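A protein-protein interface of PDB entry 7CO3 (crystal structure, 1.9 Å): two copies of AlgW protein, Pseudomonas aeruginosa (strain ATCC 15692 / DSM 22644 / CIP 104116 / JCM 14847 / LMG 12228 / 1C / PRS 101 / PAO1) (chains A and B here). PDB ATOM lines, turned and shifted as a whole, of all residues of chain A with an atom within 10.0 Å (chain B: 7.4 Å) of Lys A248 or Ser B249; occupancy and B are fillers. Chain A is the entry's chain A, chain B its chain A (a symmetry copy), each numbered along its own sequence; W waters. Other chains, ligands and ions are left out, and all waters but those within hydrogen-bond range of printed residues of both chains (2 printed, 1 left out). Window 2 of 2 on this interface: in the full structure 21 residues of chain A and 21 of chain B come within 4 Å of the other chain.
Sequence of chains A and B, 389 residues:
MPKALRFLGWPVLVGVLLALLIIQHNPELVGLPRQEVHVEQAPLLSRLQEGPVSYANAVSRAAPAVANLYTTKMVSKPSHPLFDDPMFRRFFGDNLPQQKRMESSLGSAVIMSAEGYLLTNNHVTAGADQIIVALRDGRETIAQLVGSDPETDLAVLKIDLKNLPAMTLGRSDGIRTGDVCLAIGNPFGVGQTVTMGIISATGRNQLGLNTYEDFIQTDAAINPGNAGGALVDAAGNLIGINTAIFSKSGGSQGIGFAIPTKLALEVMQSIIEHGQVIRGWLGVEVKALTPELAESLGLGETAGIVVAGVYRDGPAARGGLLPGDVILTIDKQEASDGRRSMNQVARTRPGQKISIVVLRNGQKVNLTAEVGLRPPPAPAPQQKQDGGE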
ATOM      1  N   ILE A 245     -31.217   0.879  19.552  1.00  0.00           N
ATOM      2  CA  ILE A 245     -30.628   1.916  18.722  1.00  0.00           C
ATOM      3  C   ILE A 245     -31.626   2.343  17.662  1.00  0.00           C
ATOM      4  O   ILE A 245     -32.590   1.642  17.360  1.00  0.00           O
ATOM      5  CB  ILE A 245     -29.333   1.438  18.038  1.00  0.00           C
ATOM      6  CG1 ILE A 245     -29.644   0.483  16.868  1.00  0.00           C
ATOM      7  CG2 ILE A 245     -28.392   0.799  19.065  1.00  0.00           C
ATOM      8  CD1 ILE A 245     -28.395   0.228  15.908  1.00  0.00           C
ATOM      9  N   PHE A 246     -31.375   3.500  17.090  1.00  0.00           N
ATOM     10  CA  PHE A 246     -32.072   3.934  15.891  1.00  0.00           C
ATOM     11  C   PHE A 246     -31.029   4.008  14.787  1.00  0.00           C
ATOM     12  O   PHE A 246     -29.996   4.677  14.938  1.00  0.00           O
ATOM     13  CB  PHE A 246     -32.783   5.283  16.068  1.00  0.00           C
ATOM     14  CG  PHE A 246     -33.757   5.574  14.975  1.00  0.00           C
ATOM     15  CD1 PHE A 246     -33.321   6.063  13.732  1.00  0.00           C
ATOM     16  CD2 PHE A 246     -35.106   5.314  15.153  1.00  0.00           C
ATOM     17  CE1 PHE A 246     -34.229   6.301  12.695  1.00  0.00           C
ATOM     18  CE2 PHE A 246     -36.021   5.559  14.122  1.00  0.00           C
ATOM     19  CZ  PHE A 246     -35.585   6.046  12.901  1.00  0.00           C
ATOM     20  N   SER A 247     -31.287   3.296  13.701  1.00  0.00           N
ATOM     21  CA  SER A 247     -30.305   3.200  12.645  1.00  0.00           C
ATOM     22  C   SER A 247     -30.994   2.837  11.349  1.00  0.00           C
ATOM     23  O   SER A 247     -31.944   2.058  11.341  1.00  0.00           O
ATOM     24  CB  SER A 247     -29.253   2.123  12.939  1.00  0.00           C
ATOM     25  OG  SER A 247     -28.478   1.918  11.769  1.00  0.00           O
ATOM     26  N   LYS A 248     -30.459   3.372  10.254  1.00  0.00           N
ATOM     27  CA  LYS A 248     -30.851   2.967   8.919  1.00  0.00           C
ATOM     28  C   LYS A 248     -29.906   1.937   8.316  1.00  0.00           C
ATOM     29  O   LYS A 248     -30.035   1.626   7.136  1.00  0.00           O
ATOM     30  CB  LYS A 248     -30.939   4.211   8.029  1.00  0.00           C
ATOM     31  CG  LYS A 248     -31.736   5.324   8.719  1.00  0.00           C
ATOM     32  CD  LYS A 248     -32.592   6.138   7.767  1.00  0.00           C
ATOM     33  CE  LYS A 248     -33.841   6.640   8.466  1.00  0.00           C
ATOM     34  NZ  LYS A 248     -35.040   5.814   8.153  1.00  0.00           N
ATOM     35  N   SER A 249     -28.987   1.374   9.104  1.00  0.00           N
ATOM     36  CA  SER A 249     -27.902   0.547   8.567  1.00  0.00           C
ATOM     37  C   SER A 249     -27.668  -0.771   9.295  1.00  0.00           C
ATOM     38  O   SER A 249     -26.747  -1.499   8.916  1.00  0.00           O
ATOM     39  CB  SER A 249     -26.597   1.326   8.590  1.00  0.00           C
ATOM     40  OG  SER A 249     -26.215   1.583   9.932  1.00  0.00           O
ATOM     41  N   GLY A 250     -28.431  -1.095  10.343  1.00  0.00           N
ATOM     42  CA  GLY A 250     -28.129  -2.329  11.050  1.00  0.00           C
ATOM     43  C   GLY A 250     -27.057  -2.204  12.111  1.00  0.00           C
ATOM     44  O   GLY A 250     -26.808  -3.172  12.842  1.00  0.00           O
ATOM     45  N   GLY A 251     -26.432  -1.042  12.240  1.00  0.00           N
ATOM     46  CA  GLY A 251     -25.459  -0.838  13.285  1.00  0.00           C
ATOM     47  C   GLY A 251     -25.393   0.610  13.701  1.00  0.00           C
ATOM     48  O   GLY A 251     -26.203   1.435  13.288  1.00  0.00           O
ATOM     49  N   SER A 252     -24.430   0.907  14.570  1.00  0.00           N
ATOM     50  CA  SER A 252     -24.457   2.189  15.268  1.00  0.00           C
ATOM     51  C   SER A 252     -24.356   3.348  14.276  1.00  0.00           C
ATOM     52  O   SER A 252     -23.511   3.359  13.362  1.00  0.00           O
ATOM     53  CB  SER A 252     -23.326   2.271  16.280  1.00  0.00           C
ATOM     54  OG  SER A 252     -23.460   3.495  17.007  1.00  0.00           O
ATOM     55  N   GLN A 253     -25.239   4.327  14.465  1.00  0.00           N
ATOM     56  CA  GLN A 253     -25.131   5.647  13.851  1.00  0.00           C
ATOM     57  C   GLN A 253     -25.125   6.733  14.918  1.00  0.00           C
ATOM     58  O   GLN A 253     -25.459   7.871  14.625  1.00  0.00           O
ATOM     59  CB  GLN A 253     -26.239   5.833  12.804  1.00  0.00           C
ATOM     60  CG  GLN A 253     -25.991   4.838  11.629  1.00  0.00           C
ATOM     61  CD  GLN A 253     -26.988   4.862  10.478  1.00  0.00           C
ATOM     62  OE1 GLN A 253     -28.152   5.204  10.650  1.00  0.00           O
ATOM     63  NE2 GLN A 253     -26.508   4.509   9.286  1.00  0.00           N
ATOM     64  N   GLY A 254     -24.728   6.385  16.152  1.00  0.00           N
ATOM     65  CA  GLY A 254     -24.613   7.333  17.247  1.00  0.00           C
ATOM     66  C   GLY A 254     -25.918   7.693  17.949  1.00  0.00           C
ATOM     67  O   GLY A 254     -25.934   8.665  18.704  1.00  0.00           O
ATOM     68  N   ILE A 255     -26.997   6.963  17.713  1.00  0.00           N
ATOM     69  CA  ILE A 255     -28.287   7.204  18.376  1.00  0.00           C
ATOM     70  C   ILE A 255     -28.654   5.908  19.109  1.00  0.00           C
ATOM     71  O   ILE A 255     -29.307   5.025  18.562  1.00  0.00           O
ATOM     72  CB  ILE A 255     -29.376   7.614  17.374  1.00  0.00           C
ATOM     73  CG1 ILE A 255     -28.937   8.787  16.472  1.00  0.00           C
ATOM     74  CG2 ILE A 255     -30.745   7.905  18.113  1.00  0.00           C
ATOM     75  CD1 ILE A 255     -28.677  10.018  17.176  1.00  0.00           C
ATOM     76  N   GLY A 388     -33.909  -2.412  17.236  1.00  0.00           N
ATOM     77  CA  GLY A 388     -33.696  -1.267  16.365  1.00  0.00           C
ATOM     78  C   GLY A 388     -34.981  -0.656  15.864  1.00  0.00           C
ATOM     79  O   GLY A 388     -35.758  -1.310  15.169  1.00  0.00           O
ATOM     80  N   GLU A 389     -35.215   0.596  16.211  1.00  0.00           N
ATOM     81  CA  GLU A 389     -36.281   1.354  15.576  1.00  0.00           C
ATOM     82  C   GLU A 389     -35.728   2.128  14.383  1.00  0.00           C
ATOM     83  O   GLU A 389     -34.573   1.911  13.961  1.00  0.00           O
ATOM     84  CB  GLU A 389     -36.905   2.294  16.579  1.00  0.00           C
ATOM     85  CG  GLU A 389     -35.900   2.745  17.578  1.00  0.00           C
ATOM     86  CD  GLU A 389     -36.366   3.924  18.373  1.00  0.00           C
ATOM     87  OE1 GLU A 389     -35.986   3.987  19.547  1.00  0.00           O
ATOM     88  OE2 GLU A 389     -37.147   4.751  17.855  1.00  0.00           O
ATOM     89  N   PHE B 188     -33.209  12.217  12.935  1.00  0.00           N
ATOM     90  CA  PHE B 188     -34.349  11.334  12.685  1.00  0.00           C
ATOM     91  C   PHE B 188     -35.628  11.783  13.392  1.00  0.00           C
ATOM     92  O   PHE B 188     -36.561  10.997  13.494  1.00  0.00           O
ATOM     93  CB  PHE B 188     -34.022   9.883  13.076  1.00  0.00           C
ATOM     94  CG  PHE B 188     -32.765   9.356  12.437  1.00  0.00           C
ATOM     95  CD1 PHE B 188     -32.665   9.258  11.064  1.00  0.00           C
ATOM     96  CD2 PHE B 188     -31.692   8.963  13.208  1.00  0.00           C
ATOM     97  CE1 PHE B 188     -31.494   8.771  10.453  1.00  0.00           C
ATOM     98  CE2 PHE B 188     -30.502   8.449  12.606  1.00  0.00           C
ATOM     99  CZ  PHE B 188     -30.414   8.375  11.230  1.00  0.00           C
ATOM    100  N   ASN B 223     -26.635  13.120  11.573  1.00  0.00           N
ATOM    101  CA  ASN B 223     -27.610  12.320  10.852  1.00  0.00           C
ATOM    102  C   ASN B 223     -28.640  13.185  10.155  1.00  0.00           C
ATOM    103  O   ASN B 223     -28.776  14.361  10.493  1.00  0.00           O
ATOM    104  CB  ASN B 223     -28.329  11.393  11.839  1.00  0.00           C
ATOM    105  CG  ASN B 223     -27.456  10.201  12.221  1.00  0.00           C
ATOM    106  OD1 ASN B 223     -27.260   9.313  11.397  1.00  0.00           O
ATOM    107  ND2 ASN B 223     -26.948  10.187  13.447  1.00  0.00           N
ATOM    108  N   PRO B 224     -29.389  12.637   9.184  1.00  0.00           N
ATOM    109  CA  PRO B 224     -30.572  13.365   8.671  1.00  0.00           C
ATOM    110  C   PRO B 224     -31.417  13.861   9.823  1.00  0.00           C
ATOM    111  O   PRO B 224     -31.648  13.147  10.794  1.00  0.00           O
ATOM    112  CB  PRO B 224     -31.309  12.321   7.823  1.00  0.00           C
ATOM    113  CG  PRO B 224     -30.189  11.324   7.372  1.00  0.00           C
ATOM    114  CD  PRO B 224     -29.228  11.307   8.555  1.00  0.00           C
ATOM    115  N   ILE B 245     -23.202  15.122   5.419  1.00  0.00           N
ATOM    116  CA  ILE B 245     -22.381  13.992   5.819  1.00  0.00           C
ATOM    117  C   ILE B 245     -21.922  13.238   4.585  1.00  0.00           C
ATOM    118  O   ILE B 245     -22.484  13.368   3.500  1.00  0.00           O
ATOM    119  CB  ILE B 245     -23.145  13.029   6.748  1.00  0.00           C
ATOM    120  CG1 ILE B 245     -24.165  12.187   5.957  1.00  0.00           C
ATOM    121  CG2 ILE B 245     -23.806  13.804   7.893  1.00  0.00           C
ATOM    122  CD1 ILE B 245     -24.735  10.943   6.778  1.00  0.00           C
ATOM    123  N   PHE B 246     -20.897  12.434   4.769  1.00  0.00           N
ATOM    124  CA  PHE B 246     -20.497  11.456   3.771  1.00  0.00           C
ATOM    125  C   PHE B 246     -20.727  10.087   4.392  1.00  0.00           C
ATOM    126  O   PHE B 246     -20.226   9.798   5.489  1.00  0.00           O
ATOM    127  CB  PHE B 246     -19.038  11.619   3.326  1.00  0.00           C
ATOM    128  CG  PHE B 246     -18.720  10.850   2.087  1.00  0.00           C
ATOM    129  CD1 PHE B 246     -18.459   9.471   2.143  1.00  0.00           C
ATOM    130  CD2 PHE B 246     -18.729  11.477   0.852  1.00  0.00           C
ATOM    131  CE1 PHE B 246     -18.196   8.741   0.978  1.00  0.00           C
ATOM    132  CE2 PHE B 246     -18.458  10.756  -0.317  1.00  0.00           C
ATOM    133  CZ  PHE B 246     -18.197   9.397  -0.255  1.00  0.00           C
ATOM    134  N   SER B 247     -21.510   9.267   3.707  1.00  0.00           N
ATOM    135  CA  SER B 247     -21.890   7.990   4.265  1.00  0.00           C
ATOM    136  C   SER B 247     -22.283   7.049   3.149  1.00  0.00           C
ATOM    137  O   SER B 247     -22.889   7.464   2.163  1.00  0.00           O
ATOM    138  CB  SER B 247     -23.085   8.117   5.219  1.00  0.00           C
ATOM    139  OG  SER B 247     -23.551   6.814   5.533  1.00  0.00           O
ATOM    140  N   LYS B 248     -21.977   5.771   3.352  1.00  0.00           N
ATOM    141  CA  LYS B 248     -22.464   4.708   2.495  1.00  0.00           C
ATOM    142  C   LYS B 248     -23.700   4.020   3.057  1.00  0.00           C
ATOM    143  O   LYS B 248     -24.121   3.006   2.510  1.00  0.00           O
ATOM    144  CB  LYS B 248     -21.336   3.697   2.266  1.00  0.00           C
ATOM    145  CG  LYS B 248     -20.033   4.406   1.881  1.00  0.00           C
ATOM    146  CD  LYS B 248     -19.205   3.646   0.861  1.00  0.00           C
ATOM    147  CE  LYS B 248     -18.424   4.606  -0.017  1.00  0.00           C
ATOM    148  NZ  LYS B 248     -19.070   4.820  -1.341  1.00  0.00           N
ATOM    149  N   SER B 249     -24.311   4.566   4.111  1.00  0.00           N
ATOM    150  CA  SER B 249     -25.365   3.862   4.851  1.00  0.00           C
ATOM    151  C   SER B 249     -26.609   4.689   5.154  1.00  0.00           C
ATOM    152  O   SER B 249     -27.519   4.168   5.804  1.00  0.00           O
ATOM    153  CB  SER B 249     -24.817   3.352   6.173  1.00  0.00           C
ATOM    154  OG  SER B 249     -24.470   4.449   7.005  1.00  0.00           O
ATOM    155  N   GLY B 250     -26.677   5.961   4.748  1.00  0.00           N
ATOM    156  CA  GLY B 250     -27.851   6.732   5.116  1.00  0.00           C
ATOM    157  C   GLY B 250     -27.783   7.372   6.486  1.00  0.00           C
ATOM    158  O   GLY B 250     -28.686   8.140   6.845  1.00  0.00           O
ATOM    159  N   GLY B 251     -26.733   7.109   7.252  1.00  0.00           N
ATOM    160  CA  GLY B 251     -26.574   7.752   8.533  1.00  0.00           C
ATOM    161  C   GLY B 251     -25.118   7.883   8.904  1.00  0.00           C
ATOM    162  O   GLY B 251     -24.224   7.611   8.109  1.00  0.00           O
ATOM    163  N   SER B 252     -24.885   8.350  10.129  1.00  0.00           N
ATOM    164  CA  SER B 252     -23.543   8.801  10.487  1.00  0.00           C
ATOM    165  C   SER B 252     -22.541   7.649  10.392  1.00  0.00           C
ATOM    166  O   SER B 252     -22.779   6.531  10.882  1.00  0.00           O
ATOM    167  CB  SER B 252     -23.532   9.384  11.891  1.00  0.00           C
ATOM    168  OG  SER B 252     -22.226   9.906  12.151  1.00  0.00           O
ATOM    169  N   GLN B 253     -21.415   7.939   9.745  1.00  0.00           N
ATOM    170  CA  GLN B 253     -20.213   7.113   9.800  1.00  0.00           C
ATOM    171  C   GLN B 253     -19.024   7.932  10.288  1.00  0.00           C
ATOM    172  O   GLN B 253     -17.889   7.573  10.014  1.00  0.00           O
ATOM    173  CB  GLN B 253     -19.969   6.446   8.438  1.00  0.00           C
ATOM    174  CG  GLN B 253     -21.121   5.432   8.163  1.00  0.00           C
ATOM    175  CD  GLN B 253     -21.067   4.659   6.853  1.00  0.00           C
ATOM    176  OE1 GLN B 253     -20.520   5.125   5.860  1.00  0.00           O
ATOM    177  NE2 GLN B 253     -21.633   3.453   6.865  1.00  0.00           N
HETATM  178  O   HOH W   1     -23.688   2.883   9.326  1.00  0.00           O
HETATM  179  O   HOH W   2     -28.357   1.731   5.076  1.00  0.00           O
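The side-chain amide nitrogen (NE2) of Gln A253 sits close to the backbone NH (N) of Gly B251.
NE2 of Gln A253 is in hydrogen-bond range of OG of Ser B249, 3.1 Å away.
O of Gln A253 lies within hydrogen-bond range of ND2 of Asn B223 (3.0 Å).
N of Phe A246 is in hydrogen-bond range of O of Ile A255 (3.0 Å).
The side-chain hydroxyl of Ser A249 lies within hydrogen-bond range of the backbone carbonyl oxygen of Gly A251 (3.4 Å).
N of Lys A248 is in hydrogen-bond range of OE1 of Gln A253 (3.0 Å).
The side-chain hydroxyl of Ser B249 is in hydrogen-bond range of the side-chain amide nitrogen of Gln B253 (3.0 Å).
OD1 of Asn B223 is in hydrogen-bond range of N of Ser B252 (2.9 Å).
The side-chain hydroxyl of Ser A247 sits at hydrogen-bond distance from the backbone NH of Ser A249, at 2.8 Å.
Among the printed residues, merely in contact across the chains: Phe A246 with Phe B188, Ser A249 with Ser B249, Gln A253 with Ser B252, Lys A248 with Phe B188, Lys A248 with Ser B249, Ile A255 with Asn B223 and Gln A253 with Phe B188.
Of chain B, only Phe B188 (3.7 Å) and Ser B249 (3.8 Å) come within 4 Å of Lys A248.
Printed residues of chain B within 4 Å of Ser A249: Ser B249 (3.6 Å).
No residue of chain A comes within 4 Å of Ser B247.
Lys B248 touches none of the printed residues of chain A.
Of the printed residues of chain A, Ser B249 touches Lys A248, Ser A249 and Gln A253.
No residue of chain A comes within 4 Å of Gly B250.
Of chain A, only Gln A253 (3.3 Å) comes within 4 Å of Gly B251.
Of the printed residues of chain A, Ser B252 touches Gln A253 (3.7 Å).
The nearest residue of chain A that does not touch Ser B249 is Ser A247 (6.4 Å).
The nearest printed residue of chain B that does not touch Ser A249 is Gln B253 (5.7 Å).
Of the 13 printed residues of chain A, 5 touch a printed residue of chain B.
Hydrophobic or aromatic side chains of chain A that line the printed part of chain B: Phe A246 and Ile A255.
Among the printed residues, 10 pairs touch across the chains.
Among the printed residues, no Asp or Glu carboxylate lies within 4 Å of a Lys or Arg side-chain nitrogen of the other chain.
Lys A248 touches Ser B249, but with the chains exchanged Ser A249 does not touch Lys B248 (6.8 Å).
Gln A253 touches Ser B249, but with the chains exchanged Ser A249 does not touch Gln B253 (5.7 Å).
Gln A253 touches Gly B251, but with the chains exchanged Gly A251 does not touch Gln B253 (8.1 Å).
Gln A253 touches Ser B252, but with the chains exchanged Ser A252 does not touch Gln B253 (6.1 Å).
9 positions are printed for both chains.
Water W2 lies within hydrogen-bond range of the backbone carbonyl oxygen (O) of Lys A248 and the backbone carbonyl oxygen (O) of Ser B249.
Water W1 lies within hydrogen-bond range of OG of Ser A249 (2.9 Å), OG of Ser B249 (2.9 Å), NE2 of Gln A253 (3.3 Å) and NE2 of Gln B253 (3.3 Å).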
